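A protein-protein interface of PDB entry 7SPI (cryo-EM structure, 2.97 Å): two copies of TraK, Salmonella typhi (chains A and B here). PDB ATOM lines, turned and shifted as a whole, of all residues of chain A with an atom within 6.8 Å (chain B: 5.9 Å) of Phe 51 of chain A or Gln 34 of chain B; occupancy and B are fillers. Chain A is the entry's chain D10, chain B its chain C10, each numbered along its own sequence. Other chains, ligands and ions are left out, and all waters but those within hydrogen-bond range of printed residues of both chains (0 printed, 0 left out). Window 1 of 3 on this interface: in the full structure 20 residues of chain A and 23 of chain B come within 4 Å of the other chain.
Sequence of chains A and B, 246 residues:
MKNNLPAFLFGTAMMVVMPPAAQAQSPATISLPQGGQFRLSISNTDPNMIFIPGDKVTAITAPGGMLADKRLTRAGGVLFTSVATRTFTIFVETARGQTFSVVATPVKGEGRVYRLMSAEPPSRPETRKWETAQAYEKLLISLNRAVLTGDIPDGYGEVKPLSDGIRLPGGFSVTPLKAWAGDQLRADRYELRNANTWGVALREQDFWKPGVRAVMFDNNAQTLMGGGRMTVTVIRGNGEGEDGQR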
ATOM      1  N   GLN A  25      11.584  -2.497   0.971  1.00  0.00           N
ATOM      2  CA  GLN A  25      11.972  -1.412   1.849  1.00  0.00           C
ATOM      3  C   GLN A  25      13.356  -0.938   1.467  1.00  0.00           C
ATOM      4  O   GLN A  25      13.977  -1.505   0.574  1.00  0.00           O
ATOM      5  CB  GLN A  25      11.952  -1.867   3.309  1.00  0.00           C
ATOM      6  CG  GLN A  25      11.522  -0.802   4.303  1.00  0.00           C
ATOM      7  CD  GLN A  25      11.624  -1.282   5.735  1.00  0.00           C
ATOM      8  OE1 GLN A  25      12.042  -2.410   5.994  1.00  0.00           O
ATOM      9  NE2 GLN A  25      11.243  -0.426   6.675  1.00  0.00           N
ATOM     10  N   SER A  26      13.844   0.099   2.134  1.00  0.00           N
ATOM     11  CA  SER A  26      15.148   0.645   1.831  1.00  0.00           C
ATOM     12  C   SER A  26      15.858   0.773   3.161  1.00  0.00           C
ATOM     13  O   SER A  26      15.206   0.965   4.182  1.00  0.00           O
ATOM     14  CB  SER A  26      14.968   2.009   1.175  1.00  0.00           C
ATOM     15  OG  SER A  26      16.186   2.521   0.666  1.00  0.00           O
ATOM     16  N   PRO A  27      17.191   0.646   3.175  1.00  0.00           N
ATOM     17  CA  PRO A  27      17.827   0.701   4.486  1.00  0.00           C
ATOM     18  C   PRO A  27      17.594   2.056   5.109  1.00  0.00           C
ATOM     19  O   PRO A  27      17.569   3.060   4.401  1.00  0.00           O
ATOM     20  CB  PRO A  27      19.302   0.507   4.166  1.00  0.00           C
ATOM     21  CG  PRO A  27      19.445   0.787   2.711  1.00  0.00           C
ATOM     22  CD  PRO A  27      18.152   0.347   2.106  1.00  0.00           C
ATOM     23  N   ALA A  28      17.413   2.098   6.427  1.00  0.00           N
ATOM     24  CA  ALA A  28      17.201   3.367   7.119  1.00  0.00           C
ATOM     25  C   ALA A  28      18.474   4.163   7.152  1.00  0.00           C
ATOM     26  O   ALA A  28      19.487   3.686   7.636  1.00  0.00           O
ATOM     27  CB  ALA A  28      16.684   3.140   8.513  1.00  0.00           C
ATOM     28  N   MET A  49      22.100  -5.552  10.353  1.00  0.00           N
ATOM     29  CA  MET A  49      23.228  -5.060   9.572  1.00  0.00           C
ATOM     30  C   MET A  49      23.415  -3.559   9.688  1.00  0.00           C
ATOM     31  O   MET A  49      22.446  -2.819   9.830  1.00  0.00           O
ATOM     32  CB  MET A  49      23.067  -5.458   8.100  1.00  0.00           C
ATOM     33  CG  MET A  49      24.314  -5.256   7.252  1.00  0.00           C
ATOM     34  SD  MET A  49      24.046  -5.589   5.503  1.00  0.00           S
ATOM     35  CE  MET A  49      25.668  -5.217   4.843  1.00  0.00           C
ATOM     36  N   ILE A  50      24.660  -3.107   9.634  1.00  0.00           N
ATOM     37  CA  ILE A  50      24.971  -1.692   9.700  1.00  0.00           C
ATOM     38  C   ILE A  50      26.060  -1.552   8.682  1.00  0.00           C
ATOM     39  O   ILE A  50      27.098  -2.181   8.809  1.00  0.00           O
ATOM     40  CB  ILE A  50      25.564  -1.323  11.068  1.00  0.00           C
ATOM     41  CG1 ILE A  50      24.479  -1.227  12.140  1.00  0.00           C
ATOM     42  CG2 ILE A  50      26.306  -0.001  11.003  1.00  0.00           C
ATOM     43  CD1 ILE A  50      23.820   0.127  12.230  1.00  0.00           C
ATOM     44  N   PHE A  51      25.827  -0.759   7.648  1.00  0.00           N
ATOM     45  CA  PHE A  51      26.867  -0.514   6.657  1.00  0.00           C
ATOM     46  C   PHE A  51      27.082   0.961   6.434  1.00  0.00           C
ATOM     47  O   PHE A  51      26.138   1.739   6.466  1.00  0.00           O
ATOM     48  CB  PHE A  51      26.607  -1.256   5.338  1.00  0.00           C
ATOM     49  CG  PHE A  51      25.430  -0.757   4.550  1.00  0.00           C
ATOM     50  CD1 PHE A  51      24.137  -1.042   4.944  1.00  0.00           C
ATOM     51  CD2 PHE A  51      25.625  -0.050   3.377  1.00  0.00           C
ATOM     52  CE1 PHE A  51      23.061  -0.593   4.209  1.00  0.00           C
ATOM     53  CE2 PHE A  51      24.553   0.399   2.637  1.00  0.00           C
ATOM     54  CZ  PHE A  51      23.268   0.126   3.053  1.00  0.00           C
ATOM     55  N   ILE A  52      28.330   1.359   6.259  1.00  0.00           N
ATOM     56  CA  ILE A  52      28.604   2.751   5.950  1.00  0.00           C
ATOM     57  C   ILE A  52      29.036   2.773   4.500  1.00  0.00           C
ATOM     58  O   ILE A  52      30.047   2.181   4.150  1.00  0.00           O
ATOM     59  CB  ILE A  52      29.744   3.322   6.808  1.00  0.00           C
ATOM     60  CG1 ILE A  52      29.571   2.945   8.277  1.00  0.00           C
ATOM     61  CG2 ILE A  52      29.826   4.833   6.662  1.00  0.00           C
ATOM     62  CD1 ILE A  52      30.506   1.856   8.746  1.00  0.00           C
ATOM     63  N   PRO A  53      28.260   3.433   3.642  1.00  0.00           N
ATOM     64  CA  PRO A  53      28.646   3.384   2.243  1.00  0.00           C
ATOM     65  C   PRO A  53      29.970   4.087   2.012  1.00  0.00           C
ATOM     66  O   PRO A  53      30.182   5.176   2.541  1.00  0.00           O
ATOM     67  CB  PRO A  53      27.525   4.144   1.565  1.00  0.00           C
ATOM     68  CG  PRO A  53      26.346   3.867   2.411  1.00  0.00           C
ATOM     69  CD  PRO A  53      26.868   3.869   3.814  1.00  0.00           C
ATOM     70  N   GLY A  54      30.855   3.474   1.235  1.00  0.00           N
ATOM     71  CA  GLY A  54      32.156   4.061   0.961  1.00  0.00           C
ATOM     72  C   GLY A  54      33.135   3.780   2.071  1.00  0.00           C
ATOM     73  O   GLY A  54      34.260   4.267   2.047  1.00  0.00           O
ATOM     74  N   ASP A  55      32.719   3.022   3.076  1.00  0.00           N
ATOM     75  CA  ASP A  55      33.586   2.776   4.225  1.00  0.00           C
ATOM     76  C   ASP A  55      33.540   1.338   4.690  1.00  0.00           C
ATOM     77  O   ASP A  55      32.538   0.659   4.521  1.00  0.00           O
ATOM     78  CB  ASP A  55      33.184   3.690   5.368  1.00  0.00           C
ATOM     79  CG  ASP A  55      34.370   4.304   6.058  1.00  0.00           C
ATOM     80  OD1 ASP A  55      35.481   3.743   5.957  1.00  0.00           O
ATOM     81  OD2 ASP A  55      34.189   5.353   6.708  1.00  0.00           O
ATOM     82  N   VAL A  57      33.873  -1.221   7.921  1.00  0.00           N
ATOM     83  CA  VAL A  57      33.906  -1.315   9.359  1.00  0.00           C
ATOM     84  C   VAL A  57      35.161  -2.063   9.711  1.00  0.00           C
ATOM     85  O   VAL A  57      35.406  -3.137   9.188  1.00  0.00           O
ATOM     86  CB  VAL A  57      32.699  -2.081   9.889  1.00  0.00           C
ATOM     87  CG1 VAL A  57      32.573  -1.885  11.389  1.00  0.00           C
ATOM     88  CG2 VAL A  57      31.438  -1.601   9.201  1.00  0.00           C
ATOM     89  N   THR A  73      30.619  -8.284   6.433  1.00  0.00           N
ATOM     90  CA  THR A  73      29.995  -8.562   5.152  1.00  0.00           C
ATOM     91  C   THR A  73      30.815  -8.086   3.979  1.00  0.00           C
ATOM     92  O   THR A  73      31.777  -7.347   4.148  1.00  0.00           O
ATOM     93  CB  THR A  73      28.591  -7.955   5.058  1.00  0.00           C
ATOM     94  OG1 THR A  73      28.612  -6.798   4.220  1.00  0.00           O
ATOM     95  CG2 THR A  73      28.085  -7.593   6.425  1.00  0.00           C
ATOM     96  N   ALA A  75      31.985  -5.888   0.988  1.00  0.00           N
ATOM     97  CA  ALA A  75      31.928  -4.430   0.873  1.00  0.00           C
ATOM     98  C   ALA A  75      31.627  -3.744   2.185  1.00  0.00           C
ATOM     99  O   ALA A  75      30.773  -2.862   2.237  1.00  0.00           O
ATOM    100  CB  ALA A  75      30.966  -3.980  -0.211  1.00  0.00           C
ATOM    101  N   GLY A  76      32.299  -4.156   3.255  1.00  0.00           N
ATOM    102  CA  GLY A  76      32.130  -3.492   4.530  1.00  0.00           C
ATOM    103  C   GLY A  76      30.818  -3.909   5.116  1.00  0.00           C
ATOM    104  O   GLY A  76      30.145  -4.771   4.587  1.00  0.00           O
ATOM    105  N   GLY A  77      30.424  -3.286   6.202  1.00  0.00           N
ATOM    106  CA  GLY A  77      29.196  -3.670   6.850  1.00  0.00           C
ATOM    107  C   GLY A  77      29.468  -4.679   7.925  1.00  0.00           C
ATOM    108  O   GLY A  77      30.461  -5.388   7.873  1.00  0.00           O
ATOM    109  N   VAL A  78      28.593  -4.741   8.913  1.00  0.00           N
ATOM    110  CA  VAL A  78      28.736  -5.731   9.963  1.00  0.00           C
ATOM    111  C   VAL A  78      27.430  -6.441  10.148  1.00  0.00           C
ATOM    112  O   VAL A  78      26.376  -5.819  10.134  1.00  0.00           O
ATOM    113  CB  VAL A  78      29.182  -5.151  11.319  1.00  0.00           C
ATOM    114  CG1 VAL A  78      30.664  -5.384  11.546  1.00  0.00           C
ATOM    115  CG2 VAL A  78      28.809  -3.685  11.450  1.00  0.00           C
ATOM    116  N   VAL A 113      18.200  -3.104   9.002  1.00  0.00           N
ATOM    117  CA  VAL A 113      19.424  -2.665   8.324  1.00  0.00           C
ATOM    118  C   VAL A 113      19.499  -1.160   8.285  1.00  0.00           C
ATOM    119  O   VAL A 113      18.522  -0.496   7.968  1.00  0.00           O
ATOM    120  CB  VAL A 113      19.593  -3.300   6.932  1.00  0.00           C
ATOM    121  CG1 VAL A 113      18.299  -3.241   6.139  1.00  0.00           C
ATOM    122  CG2 VAL A 113      20.760  -2.695   6.175  1.00  0.00           C
ATOM    123  N   TYR A 114      20.650  -0.619   8.660  1.00  0.00           N
ATOM    124  CA  TYR A 114      20.807   0.816   8.724  1.00  0.00           C
ATOM    125  C   TYR A 114      21.955   1.304   7.866  1.00  0.00           C
ATOM    126  O   TYR A 114      22.996   0.663   7.804  1.00  0.00           O
ATOM    127  CB  TYR A 114      20.993   1.243  10.169  1.00  0.00           C
ATOM    128  CG  TYR A 114      19.792   1.035  11.054  1.00  0.00           C
ATOM    129  CD1 TYR A 114      18.788   1.979  11.112  1.00  0.00           C
ATOM    130  CD2 TYR A 114      19.678  -0.093  11.851  1.00  0.00           C
ATOM    131  CE1 TYR A 114      17.691   1.803  11.923  1.00  0.00           C
ATOM    132  CE2 TYR A 114      18.583  -0.279  12.664  1.00  0.00           C
ATOM    133  CZ  TYR A 114      17.593   0.674  12.692  1.00  0.00           C
ATOM    134  OH  TYR A 114      16.497   0.507  13.496  1.00  0.00           O
ATOM    135  N   ARG A 115      21.760   2.429   7.188  1.00  0.00           N
ATOM    136  CA  ARG A 115      22.791   2.991   6.330  1.00  0.00           C
ATOM    137  C   ARG A 115      23.412   4.174   7.023  1.00  0.00           C
ATOM    138  O   ARG A 115      22.745   5.168   7.260  1.00  0.00           O
ATOM    139  CB  ARG A 115      22.155   3.465   5.041  1.00  0.00           C
ATOM    140  CG  ARG A 115      23.127   3.665   3.905  1.00  0.00           C
ATOM    141  CD  ARG A 115      22.394   3.780   2.584  1.00  0.00           C
ATOM    142  NE  ARG A 115      21.666   5.033   2.475  1.00  0.00           N
ATOM    143  CZ  ARG A 115      22.155   6.121   1.893  1.00  0.00           C
ATOM    144  NH1 ARG A 115      23.370   6.096   1.363  1.00  0.00           N
ATOM    145  NH2 ARG A 115      21.431   7.228   1.835  1.00  0.00           N
ATOM    146  N   LEU A 116      24.702   4.110   7.303  1.00  0.00           N
ATOM    147  CA  LEU A 116      25.325   5.168   8.079  1.00  0.00           C
ATOM    148  C   LEU A 116      25.922   6.215   7.200  1.00  0.00           C
ATOM    149  O   LEU A 116      26.692   5.916   6.304  1.00  0.00           O
ATOM    150  CB  LEU A 116      26.420   4.605   8.971  1.00  0.00           C
ATOM    151  CG  LEU A 116      26.202   4.552  10.475  1.00  0.00           C
ATOM    152  CD1 LEU A 116      25.848   5.932  11.001  1.00  0.00           C
ATOM    153  CD2 LEU A 116      25.121   3.542  10.805  1.00  0.00           C
ATOM    154  N   MET A 117      25.584   7.462   7.471  1.00  0.00           N
ATOM    155  CA  MET A 117      26.107   8.546   6.684  1.00  0.00           C
ATOM    156  C   MET A 117      26.837   9.568   7.526  1.00  0.00           C
ATOM    157  O   MET A 117      26.605   9.663   8.725  1.00  0.00           O
ATOM    158  CB  MET A 117      24.987   9.205   5.882  1.00  0.00           C
ATOM    159  CG  MET A 117      24.326   8.300   4.855  1.00  0.00           C
ATOM    160  SD  MET A 117      24.928   8.548   3.174  1.00  0.00           S
ATOM    161  CE  MET A 117      26.555   7.802   3.230  1.00  0.00           C
ATOM    162  N   LEU B  32      15.321  -4.780  -5.398  1.00  0.00           N
ATOM    163  CA  LEU B  32      15.486  -4.123  -4.112  1.00  0.00           C
ATOM    164  C   LEU B  32      16.719  -3.289  -4.140  1.00  0.00           C
ATOM    165  O   LEU B  32      17.682  -3.708  -4.734  1.00  0.00           O
ATOM    166  CB  LEU B  32      15.734  -5.180  -3.041  1.00  0.00           C
ATOM    167  CG  LEU B  32      14.643  -6.130  -2.595  1.00  0.00           C
ATOM    168  CD1 LEU B  32      15.256  -7.152  -1.657  1.00  0.00           C
ATOM    169  CD2 LEU B  32      13.515  -5.366  -1.925  1.00  0.00           C
ATOM    170  N   PRO B  33      16.732  -2.129  -3.451  1.00  0.00           N
ATOM    171  CA  PRO B  33      17.968  -1.349  -3.340  1.00  0.00           C
ATOM    172  C   PRO B  33      18.939  -2.130  -2.496  1.00  0.00           C
ATOM    173  O   PRO B  33      18.621  -3.219  -2.050  1.00  0.00           O
ATOM    174  CB  PRO B  33      17.530  -0.129  -2.572  1.00  0.00           C
ATOM    175  CG  PRO B  33      16.335  -0.563  -1.801  1.00  0.00           C
ATOM    176  CD  PRO B  33      15.622  -1.503  -2.716  1.00  0.00           C
ATOM    177  N   GLN B  34      20.120  -1.621  -2.245  1.00  0.00           N
ATOM    178  CA  GLN B  34      21.109  -2.412  -1.513  1.00  0.00           C
ATOM    179  C   GLN B  34      20.944  -2.287  -0.004  1.00  0.00           C
ATOM    180  O   GLN B  34      21.921  -2.137   0.730  1.00  0.00           O
ATOM    181  CB  GLN B  34      22.506  -1.970  -1.938  1.00  0.00           C
ATOM    182  CG  GLN B  34      22.654  -1.724  -3.431  1.00  0.00           C
ATOM    183  CD  GLN B  34      24.013  -2.124  -3.966  1.00  0.00           C
ATOM    184  OE1 GLN B  34      24.122  -2.673  -5.063  1.00  0.00           O
ATOM    185  NE2 GLN B  34      25.058  -1.848  -3.198  1.00  0.00           N
ATOM    186  N   GLY B  35      19.703  -2.352   0.468  1.00  0.00           N
ATOM    187  CA  GLY B  35      19.368  -2.492   1.869  1.00  0.00           C
ATOM    188  C   GLY B  35      18.054  -3.231   1.998  1.00  0.00           C
ATOM    189  O   GLY B  35      17.474  -3.307   3.084  1.00  0.00           O
ATOM    190  N   GLY B  36      17.583  -3.771   0.875  1.00  0.00           N
ATOM    191  CA  GLY B  36      16.183  -4.118   0.739  1.00  0.00           C
ATOM    192  C   GLY B  36      15.693  -5.108   1.777  1.00  0.00           C
ATOM    193  O   GLY B  36      16.433  -5.943   2.295  1.00  0.00           O
ATOM    194  N   GLY B  97      30.074  -7.117  -4.548  1.00  0.00           N
ATOM    195  CA  GLY B  97      29.745  -6.120  -3.551  1.00  0.00           C
ATOM    196  C   GLY B  97      28.281  -5.748  -3.598  1.00  0.00           C
ATOM    197  O   GLY B  97      27.870  -4.902  -4.398  1.00  0.00           O
ATOM    198  N   GLN B  98      27.495  -6.361  -2.717  1.00  0.00           N
ATOM    199  CA  GLN B  98      26.047  -6.217  -2.681  1.00  0.00           C
ATOM    200  C   GLN B  98      25.525  -6.970  -1.469  1.00  0.00           C
ATOM    201  O   GLN B  98      26.132  -7.950  -1.027  1.00  0.00           O
ATOM    202  CB  GLN B  98      25.390  -6.753  -3.960  1.00  0.00           C
ATOM    203  CG  GLN B  98      24.938  -5.679  -4.931  1.00  0.00           C
ATOM    204  CD  GLN B  98      24.494  -6.247  -6.262  1.00  0.00           C
ATOM    205  OE1 GLN B  98      24.717  -7.421  -6.555  1.00  0.00           O
ATOM    206  NE2 GLN B  98      23.860  -5.415  -7.078  1.00  0.00           N
ATOM    207  N   THR B  99      24.399  -6.503  -0.936  1.00  0.00           N
ATOM    208  CA  THR B  99      23.758  -7.168   0.189  1.00  0.00           C
ATOM    209  C   THR B  99      22.261  -6.915   0.122  1.00  0.00           C
ATOM    210  O   THR B  99      21.831  -5.763   0.041  1.00  0.00           O
ATOM    211  CB  THR B  99      24.316  -6.673   1.528  1.00  0.00           C
ATOM    212  OG1 THR B  99      25.730  -6.903   1.575  1.00  0.00           O
ATOM    213  CG2 THR B  99      23.650  -7.408   2.680  1.00  0.00           C
ATOM    214  N   PHE B 100      21.477  -7.989   0.154  1.00  0.00           N
ATOM    215  CA  PHE B 100      20.024  -7.895   0.138  1.00  0.00           C
ATOM    216  C   PHE B 100      19.454  -8.767   1.245  1.00  0.00           C
ATOM    217  O   PHE B 100      19.927  -9.884   1.463  1.00  0.00           O
ATOM    218  CB  PHE B 100      19.449  -8.315  -1.219  1.00  0.00           C
ATOM    219  CG  PHE B 100      20.207  -7.769  -2.397  1.00  0.00           C
ATOM    220  CD1 PHE B 100      20.125  -6.428  -2.728  1.00  0.00           C
ATOM    221  CD2 PHE B 100      21.000  -8.597  -3.173  1.00  0.00           C
ATOM    222  CE1 PHE B 100      20.815  -5.924  -3.812  1.00  0.00           C
ATOM    223  CE2 PHE B 100      21.695  -8.097  -4.255  1.00  0.00           C
ATOM    224  CZ  PHE B 100      21.600  -6.759  -4.575  1.00  0.00           C
ATOM    225  N   SER B 118      18.979  -5.418  -8.977  1.00  0.00           N
ATOM    226  CA  SER B 118      19.665  -4.509  -8.076  1.00  0.00           C
ATOM    227  C   SER B 118      19.037  -3.199  -7.695  1.00  0.00           C
ATOM    228  O   SER B 118      19.243  -2.764  -6.574  1.00  0.00           O
ATOM    229  CB  SER B 118      21.056  -4.243  -8.567  1.00  0.00           C
ATOM    230  OG  SER B 118      21.006  -3.428  -9.707  1.00  0.00           O
ATOM    231  N   GLU B 120      19.893  -0.443  -7.572  1.00  0.00           N
ATOM    232  CA  GLU B 120      20.994   0.503  -7.533  1.00  0.00           C
ATOM    233  C   GLU B 120      22.145  -0.253  -8.127  1.00  0.00           C
ATOM    234  O   GLU B 120      22.644  -1.172  -7.504  1.00  0.00           O
ATOM    235  CB  GLU B 120      21.346   0.842  -6.106  1.00  0.00           C
ATOM    236  CG  GLU B 120      20.253   1.544  -5.324  1.00  0.00           C
ATOM    237  CD  GLU B 120      20.707   1.954  -3.938  1.00  0.00           C
ATOM    238  OE1 GLU B 120      19.941   2.652  -3.242  1.00  0.00           O
ATOM    239  OE2 GLU B 120      21.834   1.586  -3.546  1.00  0.00           O
ATOM    240  N   PRO B 121      22.635   0.164  -9.293  1.00  0.00           N
ATOM    241  CA  PRO B 121      23.681  -0.601  -9.973  1.00  0.00           C
ATOM    242  C   PRO B 121      24.978  -0.735  -9.202  1.00  0.00           C
ATOM    243  O   PRO B 121      25.379   0.192  -8.524  1.00  0.00           O
ATOM    244  CB  PRO B 121      23.927   0.224 -11.219  1.00  0.00           C
ATOM    245  CG  PRO B 121      22.631   0.891 -11.496  1.00  0.00           C
ATOM    246  CD  PRO B 121      22.062   1.214 -10.151  1.00  0.00           C
ATOM    247  N   PRO B 122      25.622  -1.891  -9.270  1.00  0.00           N
ATOM    248  CA  PRO B 122      26.884  -2.131  -8.574  1.00  0.00           C
ATOM    249  C   PRO B 122      28.105  -1.510  -9.189  1.00  0.00           C
ATOM    250  O   PRO B 122      28.136  -1.326 -10.391  1.00  0.00           O
ATOM    251  CB  PRO B 122      27.034  -3.644  -8.659  1.00  0.00           C
ATOM    252  CG  PRO B 122      26.243  -4.054  -9.841  1.00  0.00           C
ATOM    253  CD  PRO B 122      25.080  -3.116  -9.874  1.00  0.00           C
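Of the 22 printed residues of chain A, 7 touch a printed residue of chain B. Of the 13 printed residues of chain B, 5 touch a printed residue of chain A. Printed residues of chain B that touch a printed residue of chain A: Pro 33, Gln 34, Gly 35, Gly 36 and Thr 99. Among the printed residues, no Asp or Glu carboxylate lies within 4 Å of a Lys or Arg side-chain nitrogen of the other chain.
Among the printed residues, pairs that only touch across the chains: Pro 27 of chain A with Gly 35 of chain B, Val 113 of chain A with Gly 35 of chain B, Met 49 of chain A with Thr 99 of chain B, Gln 25 of chain A with Gly 36 of chain B, Gln 25 of chain A with Pro 33 of chain B, Phe 51 of chain A with Gln 34 of chain B, Thr 73 of chain A with Thr 99 of chain B and Ser 26 of chain A with Pro 33 of chain B.
Printed residues of chain B within 4 Å of Pro 27 of chain A: Gly 35 (3.1 Å). Of the printed residues of chain B, Met 49 of chain A touches Thr 99. Phe 51 of chain A touches just one residue of chain B: Gln 34. Printed residues of chain B within 4 Å of Val 113 of chain A: Gly 35 (3.2 Å). Met 117 of chain A touches none of the printed residues of chain B. Of chain A, only Phe 51 (3.5 Å) comes within 4 Å of Gln 34 of chain B. Of the printed residues of chain A, Gly 36 of chain B touches Gln 25. The nearest residue of chain B that does not touch Phe 51 of chain A is Gly 35 of chain B (4.8 Å). The nearest printed residue of chain B that does not touch Met 49 of chain A is Gln 34 of chain B (6.3 Å).
No position is printed for both chains.
O of Glu 120 of chain B sits close to OE1 of Gln 34 of chain B (3.2 Å). The backbone NH (N) of Tyr 114 of chain A is in hydrogen-bond range of the backbone carbonyl oxygen (O) of Met 49 of chain A (3.1 Å). The side-chain amide oxygen (OE1) of Gln 34 of chain B lies close to the side-chain amide nitrogen (NE2) of Gln 98 of chain B, at 3.4 Å. O of Gly 76 of chain A lies within hydrogen-bond range of OG1 of Thr 73 of chain A. The backbone NH (N) of Leu 116 of chain A sits at hydrogen-bond distance from the backbone carbonyl oxygen (O) of Phe 51 of chain A (2.9 Å). N of Phe 51 of chain A is in hydrogen-bond range of O of Tyr 114 of chain A (3.2 Å).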
